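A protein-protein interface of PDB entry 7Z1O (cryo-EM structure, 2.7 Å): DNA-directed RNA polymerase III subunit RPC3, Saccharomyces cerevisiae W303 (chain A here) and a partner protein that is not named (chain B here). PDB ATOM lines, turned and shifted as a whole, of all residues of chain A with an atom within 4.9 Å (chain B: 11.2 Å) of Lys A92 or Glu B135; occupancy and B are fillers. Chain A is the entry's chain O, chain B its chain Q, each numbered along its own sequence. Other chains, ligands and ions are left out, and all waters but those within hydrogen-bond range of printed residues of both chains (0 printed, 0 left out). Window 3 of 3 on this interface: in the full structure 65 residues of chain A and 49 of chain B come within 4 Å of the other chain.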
ATOM      1  N   VAL A  76      11.608   3.996   9.007  1.00  0.00           N
ATOM      2  CA  VAL A  76      12.061   4.172  10.383  1.00  0.00           C
ATOM      3  C   VAL A  76      13.371   3.427  10.606  1.00  0.00           C
ATOM      4  O   VAL A  76      14.301   3.947  11.237  1.00  0.00           O
ATOM      5  CB  VAL A  76      10.970   3.715  11.369  1.00  0.00           C
ATOM      6  CG1 VAL A  76      11.467   3.809  12.799  1.00  0.00           C
ATOM      7  CG2 VAL A  76       9.714   4.548  11.188  1.00  0.00           C
ATOM      8  N   VAL A  88      15.007   3.467  17.815  1.00  0.00           N
ATOM      9  CA  VAL A  88      13.713   3.370  17.144  1.00  0.00           C
ATOM     10  C   VAL A  88      12.671   4.240  17.837  1.00  0.00           C
ATOM     11  O   VAL A  88      11.889   4.939  17.177  1.00  0.00           O
ATOM     12  CB  VAL A  88      13.267   1.899  17.071  1.00  0.00           C
ATOM     13  CG1 VAL A  88      11.931   1.777  16.359  1.00  0.00           C
ATOM     14  CG2 VAL A  88      14.330   1.066  16.377  1.00  0.00           C
ATOM     15  N   ASP A  89      12.641   4.215  19.172  1.00  0.00           N
ATOM     16  CA  ASP A  89      11.640   4.986  19.904  1.00  0.00           C
ATOM     17  C   ASP A  89      11.850   6.486  19.732  1.00  0.00           C
ATOM     18  O   ASP A  89      10.883   7.241  19.578  1.00  0.00           O
ATOM     19  CB  ASP A  89      11.661   4.601  21.383  1.00  0.00           C
ATOM     20  CG  ASP A  89      11.050   3.237  21.639  1.00  0.00           C
ATOM     21  OD1 ASP A  89      10.076   2.881  20.941  1.00  0.00           O
ATOM     22  OD2 ASP A  89      11.537   2.521  22.539  1.00  0.00           O
ATOM     23  N   SER A  90      13.108   6.935  19.747  1.00  0.00           N
ATOM     24  CA  SER A  90      13.399   8.351  19.543  1.00  0.00           C
ATOM     25  C   SER A  90      12.994   8.812  18.147  1.00  0.00           C
ATOM     26  O   SER A  90      12.407   9.891  17.985  1.00  0.00           O
ATOM     27  CB  SER A  90      14.885   8.613  19.782  1.00  0.00           C
ATOM     28  OG  SER A  90      15.183   9.993  19.699  1.00  0.00           O
ATOM     29  N   VAL A  91      13.298   8.001  17.129  1.00  0.00           N
ATOM     30  CA  VAL A  91      12.928   8.340  15.757  1.00  0.00           C
ATOM     31  C   VAL A  91      11.412   8.372  15.607  1.00  0.00           C
ATOM     32  O   VAL A  91      10.860   9.262  14.953  1.00  0.00           O
ATOM     33  CB  VAL A  91      13.583   7.354  14.770  1.00  0.00           C
ATOM     34  CG1 VAL A  91      12.996   7.508  13.384  1.00  0.00           C
ATOM     35  CG2 VAL A  91      15.081   7.576  14.725  1.00  0.00           C
ATOM     36  N   LYS A  92      10.714   7.417  16.225  1.00  0.00           N
ATOM     37  CA  LYS A  92       9.255   7.413  16.168  1.00  0.00           C
ATOM     38  C   LYS A  92       8.666   8.640  16.855  1.00  0.00           C
ATOM     39  O   LYS A  92       7.713   9.244  16.347  1.00  0.00           O
ATOM     40  CB  LYS A  92       8.711   6.129  16.793  1.00  0.00           C
ATOM     41  CG  LYS A  92       8.620   4.966  15.820  1.00  0.00           C
ATOM     42  CD  LYS A  92       8.655   3.633  16.537  1.00  0.00           C
ATOM     43  CE  LYS A  92       8.119   2.523  15.653  1.00  0.00           C
ATOM     44  NZ  LYS A  92       7.442   1.463  16.446  1.00  0.00           N
ATOM     45  N   THR A  93       9.231   9.037  17.999  1.00  0.00           N
ATOM     46  CA  THR A  93       8.729  10.206  18.716  1.00  0.00           C
ATOM     47  C   THR A  93       8.932  11.485  17.908  1.00  0.00           C
ATOM     48  O   THR A  93       8.017  12.313  17.791  1.00  0.00           O
ATOM     49  CB  THR A  93       9.415  10.317  20.078  1.00  0.00           C
ATOM     50  OG1 THR A  93       9.216   9.104  20.814  1.00  0.00           O
ATOM     51  CG2 THR A  93       8.846  11.482  20.870  1.00  0.00           C
ATOM     52  N   THR A  94      10.121  11.658  17.324  1.00  0.00           N
ATOM     53  CA  THR A  94      10.350  12.873  16.548  1.00  0.00           C
ATOM     54  C   THR A  94       9.581  12.850  15.231  1.00  0.00           C
ATOM     55  O   THR A  94       9.204  13.912  14.721  1.00  0.00           O
ATOM     56  CB  THR A  94      11.844  13.099  16.309  1.00  0.00           C
ATOM     57  OG1 THR A  94      12.031  14.333  15.606  1.00  0.00           O
ATOM     58  CG2 THR A  94      12.453  11.983  15.504  1.00  0.00           C
ATOM     59  N   LEU A  95       9.295  11.663  14.687  1.00  0.00           N
ATOM     60  CA  LEU A  95       8.436  11.585  13.513  1.00  0.00           C
ATOM     61  C   LEU A  95       7.003  11.961  13.856  1.00  0.00           C
ATOM     62  O   LEU A  95       6.320  12.600  13.052  1.00  0.00           O
ATOM     63  CB  LEU A  95       8.493  10.186  12.904  1.00  0.00           C
ATOM     64  CG  LEU A  95       9.656   9.917  11.949  1.00  0.00           C
ATOM     65  CD1 LEU A  95       9.782   8.433  11.670  1.00  0.00           C
ATOM     66  CD2 LEU A  95       9.485  10.695  10.661  1.00  0.00           C
ATOM     67  N   VAL A  96       6.535  11.580  15.047  1.00  0.00           N
ATOM     68  CA  VAL A  96       5.218  12.017  15.508  1.00  0.00           C
ATOM     69  C   VAL A  96       5.184  13.535  15.642  1.00  0.00           C
ATOM     70  O   VAL A  96       4.233  14.198  15.204  1.00  0.00           O
ATOM     71  CB  VAL A  96       4.860  11.326  16.836  1.00  0.00           C
ATOM     72  CG1 VAL A  96       3.728  12.056  17.536  1.00  0.00           C
ATOM     73  CG2 VAL A  96       4.490   9.879  16.591  1.00  0.00           C
ATOM     74  N   THR A 118       6.161   1.680   5.751  1.00  0.00           N
ATOM     75  CA  THR A 118       5.816   3.093   5.698  1.00  0.00           C
ATOM     76  C   THR A 118       7.063   3.897   5.361  1.00  0.00           C
ATOM     77  O   THR A 118       8.080   3.792   6.053  1.00  0.00           O
ATOM     78  CB  THR A 118       5.227   3.567   7.028  1.00  0.00           C
ATOM     79  OG1 THR A 118       4.085   2.768   7.358  1.00  0.00           O
ATOM     80  CG2 THR A 118       4.809   5.023   6.936  1.00  0.00           C
ATOM     81  N   TYR A 120       8.629   7.685   4.781  1.00  0.00           N
ATOM     82  CA  TYR A 120       8.400   9.068   5.172  1.00  0.00           C
ATOM     83  C   TYR A 120       9.125  10.012   4.224  1.00  0.00           C
ATOM     84  O   TYR A 120      10.306   9.821   3.922  1.00  0.00           O
ATOM     85  CB  TYR A 120       8.865   9.311   6.608  1.00  0.00           C
ATOM     86  CG  TYR A 120       8.051   8.574   7.643  1.00  0.00           C
ATOM     87  CD1 TYR A 120       8.397   7.293   8.042  1.00  0.00           C
ATOM     88  CD2 TYR A 120       6.932   9.157   8.217  1.00  0.00           C
ATOM     89  CE1 TYR A 120       7.655   6.614   8.986  1.00  0.00           C
ATOM     90  CE2 TYR A 120       6.184   8.487   9.160  1.00  0.00           C
ATOM     91  CZ  TYR A 120       6.550   7.216   9.540  1.00  0.00           C
ATOM     92  OH  TYR A 120       5.807   6.544  10.482  1.00  0.00           O
ATOM     93  N   PRO B  69       4.371  21.134  23.329  1.00  0.00           N
ATOM     94  CA  PRO B  69       4.494  19.678  23.509  1.00  0.00           C
ATOM     95  C   PRO B  69       5.337  18.995  22.448  1.00  0.00           C
ATOM     96  O   PRO B  69       5.812  17.878  22.683  1.00  0.00           O
ATOM     97  CB  PRO B  69       3.038  19.196  23.463  1.00  0.00           C
ATOM     98  CG  PRO B  69       2.317  20.244  22.691  1.00  0.00           C
ATOM     99  CD  PRO B  69       2.993  21.543  23.010  1.00  0.00           C
ATOM    100  N   PHE B  70       5.539  19.621  21.293  1.00  0.00           N
ATOM    101  CA  PHE B  70       6.319  19.047  20.200  1.00  0.00           C
ATOM    102  C   PHE B  70       7.597  19.870  20.059  1.00  0.00           C
ATOM    103  O   PHE B  70       7.652  20.828  19.287  1.00  0.00           O
ATOM    104  CB  PHE B  70       5.518  19.039  18.903  1.00  0.00           C
ATOM    105  CG  PHE B  70       4.078  18.671  19.085  1.00  0.00           C
ATOM    106  CD1 PHE B  70       3.714  17.370  19.378  1.00  0.00           C
ATOM    107  CD2 PHE B  70       3.088  19.629  18.972  1.00  0.00           C
ATOM    108  CE1 PHE B  70       2.389  17.031  19.550  1.00  0.00           C
ATOM    109  CE2 PHE B  70       1.761  19.297  19.143  1.00  0.00           C
ATOM    110  CZ  PHE B  70       1.412  17.995  19.436  1.00  0.00           C
ATOM    111  N   THR B  72      11.198  18.092  20.973  1.00  0.00           N
ATOM    112  CA  THR B  72      12.200  17.066  20.659  1.00  0.00           C
ATOM    113  C   THR B  72      13.600  17.668  20.552  1.00  0.00           C
ATOM    114  O   THR B  72      14.222  17.683  19.491  1.00  0.00           O
ATOM    115  CB  THR B  72      11.838  16.298  19.383  1.00  0.00           C
ATOM    116  OG1 THR B  72      11.860  17.181  18.255  1.00  0.00           O
ATOM    117  CG2 THR B  72      10.455  15.681  19.510  1.00  0.00           C
ATOM    118  N   ILE B 122       5.030  14.106  24.931  1.00  0.00           N
ATOM    119  CA  ILE B 122       4.599  13.812  23.568  1.00  0.00           C
ATOM    120  C   ILE B 122       3.321  12.978  23.575  1.00  0.00           C
ATOM    121  O   ILE B 122       2.548  12.993  22.609  1.00  0.00           O
ATOM    122  CB  ILE B 122       5.739  13.123  22.791  1.00  0.00           C
ATOM    123  CG1 ILE B 122       5.443  13.088  21.291  1.00  0.00           C
ATOM    124  CG2 ILE B 122       6.004  11.721  23.328  1.00  0.00           C
ATOM    125  CD1 ILE B 122       5.424  14.450  20.646  1.00  0.00           C
ATOM    126  N   ASP B 123       3.063  12.256  24.667  1.00  0.00           N
ATOM    127  CA  ASP B 123       1.913  11.369  24.759  1.00  0.00           C
ATOM    128  C   ASP B 123       0.743  11.992  25.511  1.00  0.00           C
ATOM    129  O   ASP B 123      -0.199  11.279  25.875  1.00  0.00           O
ATOM    130  CB  ASP B 123       2.318  10.045  25.412  1.00  0.00           C
ATOM    131  CG  ASP B 123       3.010  10.236  26.748  1.00  0.00           C
ATOM    132  OD1 ASP B 123       3.273  11.396  27.129  1.00  0.00           O
ATOM    133  OD2 ASP B 123       3.295   9.222  27.419  1.00  0.00           O
ATOM    134  N   TYR B 127      -4.338  13.473  19.876  1.00  0.00           N
ATOM    135  CA  TYR B 127      -3.980  13.197  18.492  1.00  0.00           C
ATOM    136  C   TYR B 127      -5.187  12.720  17.695  1.00  0.00           C
ATOM    137  O   TYR B 127      -6.064  12.027  18.215  1.00  0.00           O
ATOM    138  CB  TYR B 127      -2.878  12.142  18.428  1.00  0.00           C
ATOM    139  CG  TYR B 127      -1.540  12.610  18.942  1.00  0.00           C
ATOM    140  CD1 TYR B 127      -0.919  13.725  18.400  1.00  0.00           C
ATOM    141  CD2 TYR B 127      -0.896  11.932  19.964  1.00  0.00           C
ATOM    142  CE1 TYR B 127       0.307  14.153  18.866  1.00  0.00           C
ATOM    143  CE2 TYR B 127       0.327  12.352  20.436  1.00  0.00           C
ATOM    144  CZ  TYR B 127       0.925  13.463  19.884  1.00  0.00           C
ATOM    145  OH  TYR B 127       2.146  13.886  20.352  1.00  0.00           O
ATOM    146  N   LEU B 129      -5.945  10.141  15.248  1.00  0.00           N
ATOM    147  CA  LEU B 129      -5.259   8.911  14.872  1.00  0.00           C
ATOM    148  C   LEU B 129      -5.451   8.537  13.408  1.00  0.00           C
ATOM    149  O   LEU B 129      -4.764   7.630  12.927  1.00  0.00           O
ATOM    150  CB  LEU B 129      -5.727   7.763  15.767  1.00  0.00           C
ATOM    151  CG  LEU B 129      -4.794   7.396  16.923  1.00  0.00           C
ATOM    152  CD1 LEU B 129      -4.720   8.518  17.945  1.00  0.00           C
ATOM    153  CD2 LEU B 129      -5.242   6.098  17.580  1.00  0.00           C
ATOM    154  N   ASN B 130      -6.358   9.201  12.689  1.00  0.00           N
ATOM    155  CA  ASN B 130      -6.521   8.934  11.266  1.00  0.00           C
ATOM    156  C   ASN B 130      -5.408   9.535  10.420  1.00  0.00           C
ATOM    157  O   ASN B 130      -5.265   9.152   9.255  1.00  0.00           O
ATOM    158  CB  ASN B 130      -7.873   9.463  10.783  1.00  0.00           C
ATOM    159  CG  ASN B 130      -9.036   8.891  11.566  1.00  0.00           C
ATOM    160  OD1 ASN B 130      -9.936   9.619  11.983  1.00  0.00           O
ATOM    161  ND2 ASN B 130      -9.024   7.580  11.771  1.00  0.00           N
ATOM    162  N   LEU B 131      -4.624  10.460  10.970  1.00  0.00           N
ATOM    163  CA  LEU B 131      -3.568  11.137  10.231  1.00  0.00           C
ATOM    164  C   LEU B 131      -2.191  10.532  10.461  1.00  0.00           C
ATOM    165  O   LEU B 131      -1.213  11.022   9.888  1.00  0.00           O
ATOM    166  CB  LEU B 131      -3.532  12.620  10.609  1.00  0.00           C
ATOM    167  CG  LEU B 131      -4.872  13.349  10.668  1.00  0.00           C
ATOM    168  CD1 LEU B 131      -4.710  14.681  11.375  1.00  0.00           C
ATOM    169  CD2 LEU B 131      -5.433  13.544   9.276  1.00  0.00           C
ATOM    170  N   PHE B 132      -2.084   9.488  11.277  1.00  0.00           N
ATOM    171  CA  PHE B 132      -0.784   8.952  11.640  1.00  0.00           C
ATOM    172  C   PHE B 132      -0.654   7.501  11.199  1.00  0.00           C
ATOM    173  O   PHE B 132      -1.648   6.771  11.150  1.00  0.00           O
ATOM    174  CB  PHE B 132      -0.557   9.044  13.154  1.00  0.00           C
ATOM    175  CG  PHE B 132      -0.295  10.437  13.645  1.00  0.00           C
ATOM    176  CD1 PHE B 132      -1.341  11.310  13.884  1.00  0.00           C
ATOM    177  CD2 PHE B 132       0.998  10.873  13.869  1.00  0.00           C
ATOM    178  CE1 PHE B 132      -1.102  12.590  14.334  1.00  0.00           C
ATOM    179  CE2 PHE B 132       1.243  12.152  14.320  1.00  0.00           C
ATOM    180  CZ  PHE B 132       0.191  13.011  14.553  1.00  0.00           C
ATOM    181  N   PRO B 133       0.556   7.059  10.860  1.00  0.00           N
ATOM    182  CA  PRO B 133       0.759   5.648  10.521  1.00  0.00           C
ATOM    183  C   PRO B 133       0.557   4.750  11.733  1.00  0.00           C
ATOM    184  O   PRO B 133       0.637   5.181  12.884  1.00  0.00           O
ATOM    185  CB  PRO B 133       2.210   5.601  10.028  1.00  0.00           C
ATOM    186  CG  PRO B 133       2.533   7.001   9.649  1.00  0.00           C
ATOM    187  CD  PRO B 133       1.751   7.870  10.577  1.00  0.00           C
ATOM    188  N   ASN B 134       0.282   3.474  11.451  1.00  0.00           N
ATOM    189  CA  ASN B 134      -0.020   2.526  12.517  1.00  0.00           C
ATOM    190  C   ASN B 134       1.201   2.217  13.375  1.00  0.00           C
ATOM    191  O   ASN B 134       1.055   1.799  14.528  1.00  0.00           O
ATOM    192  CB  ASN B 134      -0.584   1.235  11.923  1.00  0.00           C
ATOM    193  CG  ASN B 134      -1.778   1.480  11.024  1.00  0.00           C
ATOM    194  OD1 ASN B 134      -1.861   0.938   9.923  1.00  0.00           O
ATOM    195  ND2 ASN B 134      -2.711   2.301  11.491  1.00  0.00           N
ATOM    196  N   GLU B 135       2.409   2.417  12.840  1.00  0.00           N
ATOM    197  CA  GLU B 135       3.607   2.066  13.593  1.00  0.00           C
ATOM    198  C   GLU B 135       3.970   3.114  14.636  1.00  0.00           C
ATOM    199  O   GLU B 135       4.815   2.844  15.495  1.00  0.00           O
ATOM    200  CB  GLU B 135       4.789   1.852  12.647  1.00  0.00           C
ATOM    201  CG  GLU B 135       5.430   3.132  12.147  1.00  0.00           C
ATOM    202  CD  GLU B 135       6.471   2.877  11.079  1.00  0.00           C
ATOM    203  OE1 GLU B 135       7.310   1.971  11.269  1.00  0.00           O
ATOM    204  OE2 GLU B 135       6.461   3.588  10.055  1.00  0.00           O
ATOM    205  N   LEU B 136       3.359   4.293  14.585  1.00  0.00           N
ATOM    206  CA  LEU B 136       3.634   5.351  15.548  1.00  0.00           C
ATOM    207  C   LEU B 136       2.688   5.329  16.741  1.00  0.00           C
ATOM    208  O   LEU B 136       2.829   6.167  17.636  1.00  0.00           O
ATOM    209  CB  LEU B 136       3.561   6.720  14.866  1.00  0.00           C
ATOM    210  CG  LEU B 136       4.450   6.946  13.643  1.00  0.00           C
ATOM    211  CD1 LEU B 136       4.341   8.380  13.165  1.00  0.00           C
ATOM    212  CD2 LEU B 136       5.890   6.599  13.955  1.00  0.00           C
ATOM    213  N   TYR B 137       1.738   4.389  16.778  1.00  0.00           N
ATOM    214  CA  TYR B 137       0.746   4.360  17.849  1.00  0.00           C
ATOM    215  C   TYR B 137       1.366   4.020  19.199  1.00  0.00           C
ATOM    216  O   TYR B 137       0.809   4.381  20.241  1.00  0.00           O
ATOM    217  CB  TYR B 137      -0.355   3.351  17.522  1.00  0.00           C
ATOM    218  CG  TYR B 137      -1.344   3.812  16.477  1.00  0.00           C
ATOM    219  CD1 TYR B 137      -1.375   5.131  16.055  1.00  0.00           C
ATOM    220  CD2 TYR B 137      -2.249   2.925  15.912  1.00  0.00           C
ATOM    221  CE1 TYR B 137      -2.276   5.556  15.102  1.00  0.00           C
ATOM    222  CE2 TYR B 137      -3.155   3.339  14.958  1.00  0.00           C
ATOM    223  CZ  TYR B 137      -3.164   4.657  14.557  1.00  0.00           C
ATOM    224  OH  TYR B 137      -4.063   5.077  13.606  1.00  0.00           O
ATOM    225  N   ASN B 138       2.505   3.325  19.201  1.00  0.00           N
ATOM    226  CA  ASN B 138       3.084   2.847  20.452  1.00  0.00           C
ATOM    227  C   ASN B 138       3.627   3.992  21.297  1.00  0.00           C
ATOM    228  O   ASN B 138       3.606   3.926  22.531  1.00  0.00           O
ATOM    229  CB  ASN B 138       4.188   1.830  20.161  1.00  0.00           C
ATOM    230  CG  ASN B 138       3.648   0.526  19.614  1.00  0.00           C
ATOM    231  OD1 ASN B 138       2.631   0.016  20.083  1.00  0.00           O
ATOM    232  ND2 ASN B 138       4.328  -0.023  18.614  1.00  0.00           N
ATOM    233  N   VAL B 139       4.120   5.055  20.651  1.00  0.00           N
ATOM    234  CA  VAL B 139       4.815   6.117  21.371  1.00  0.00           C
ATOM    235  C   VAL B 139       3.933   7.321  21.668  1.00  0.00           C
ATOM    236  O   VAL B 139       4.384   8.247  22.356  1.00  0.00           O
ATOM    237  CB  VAL B 139       6.062   6.579  20.590  1.00  0.00           C
ATOM    238  CG1 VAL B 139       7.045   5.431  20.441  1.00  0.00           C
ATOM    239  CG2 VAL B 139       5.661   7.126  19.231  1.00  0.00           C
ATOM    240  N   MET B 140       2.694   7.346  21.181  1.00  0.00           N
ATOM    241  CA  MET B 140       1.806   8.475  21.422  1.00  0.00           C
ATOM    242  C   MET B 140       0.882   8.269  22.615  1.00  0.00           C
ATOM    243  O   MET B 140       0.170   9.204  22.995  1.00  0.00           O
ATOM    244  CB  MET B 140       0.971   8.785  20.179  1.00  0.00           C
ATOM    245  CG  MET B 140       1.774   9.291  19.001  1.00  0.00           C
ATOM    246  SD  MET B 140       0.749   9.714  17.581  1.00  0.00           S
ATOM    247  CE  MET B 140       0.303   8.096  16.979  1.00  0.00           C
ATOM    248  N   GLY B 141       0.881   7.082  23.218  1.00  0.00           N
ATOM    249  CA  GLY B 141       0.004   6.824  24.346  1.00  0.00           C
ATOM    250  C   GLY B 141      -1.462   6.911  23.972  1.00  0.00           C
ATOM    251  O   GLY B 141      -2.148   7.857  24.369  1.00  0.00           O
ATOM    252  N   ILE B 142      -1.939   5.940  23.188  1.00  0.00           N
ATOM    253  CA  ILE B 142      -3.289   6.008  22.632  1.00  0.00           C
ATOM    254  C   ILE B 142      -4.340   5.975  23.736  1.00  0.00           C
ATOM    255  O   ILE B 142      -5.440   6.520  23.580  1.00  0.00           O
ATOM    256  CB  ILE B 142      -3.501   4.876  21.609  1.00  0.00           C
ATOM    257  CG1 ILE B 142      -3.141   3.521  22.221  1.00  0.00           C
ATOM    258  CG2 ILE B 142      -2.681   5.133  20.356  1.00  0.00           C
ATOM    259  CD1 ILE B 142      -3.511   2.342  21.350  1.00  0.00           C
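The side-chain amino group of Lys A92 sits at hydrogen-bond distance from the backbone carbonyl oxygen of Glu B135 (3.1 Å). The side-chain carboxylate (OE2) of Glu B135 is in hydrogen-bond range of the side-chain hydroxyl (OH) of Tyr A120 (3.1 Å).
Lys A92 touches just these residues of chain B: Glu B135 and Leu B136. No residue of chain B comes within 4 Å of Ser A90. No residue of chain B comes within 4 Å of Val A91. Thr A93 touches one residue of chain B. Of chain B, only Thr B72 comes within 4 Å of Thr A94. Of chain B, only Glu B135 comes within 4 Å of Thr A118. Printed residues of chain A within 4 Å of Tyr B127: Val A96 (3.7 Å). Printed residues of chain A within 4 Å of Met B140: Val A96. Of the printed residues of chain B, Tyr A120 touches Pro B133, Glu B135 and Leu B136. Of the printed residues of chain A, Ile B122 touches Thr A93. Of the printed residues of chain A, Phe B132 touches Val A96 (3.7 Å). Phe B70 touches none of the printed residues of chain A. The nearest residue of chain B that does not touch Lys A92 is Val B139 (4.03 Å). The nearest printed residue of chain A that does not touch Glu B135 is Leu A95 (6.1 Å). The nearest printed residue of chain B that does not touch Asp A89 is Asn B138 (6.0 Å).
OG1 of Thr A93 sits at hydrogen-bond distance from O of Asp A89 (2.8 Å). OH of Tyr B127 is in hydrogen-bond range of O of Ile B122, 2.5 Å away.
Of the 12 printed residues of chain A, 8 touch a printed residue of chain B. Hydrophobic or aromatic side chains of chain A that line the printed part of chain B: Val A76, Val A96 and Tyr A120. Along chain A the printed residues that touch a printed residue of chain B span positions 76 to 120. Among the printed residues, 15 pairs touch across the chains.
Among the printed residues, merely in contact across the chains: Val A76 with Glu B135 (3.5 Å), Asp A89 with Val B139 (3.99 Å), Lys A92 with Leu B136 (3.7 Å), Thr A93 with Ile B122 (3.8 Å), Thr A94 with Thr B72 (3.9 Å), Val A96 with Tyr B127 (3.7 Å), Val A96 with Phe B132 (3.7 Å), Val A96 with Leu B136 (3.7 Å), Val A96 with Val B139 (3.99 Å), Val A96 with Met B140 (3.7 Å), Thr A118 with Glu B135 (3.3 Å), Tyr A120 with Pro B133 (3.4 Å) and Tyr A120 with Leu B136 (3.5 Å).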
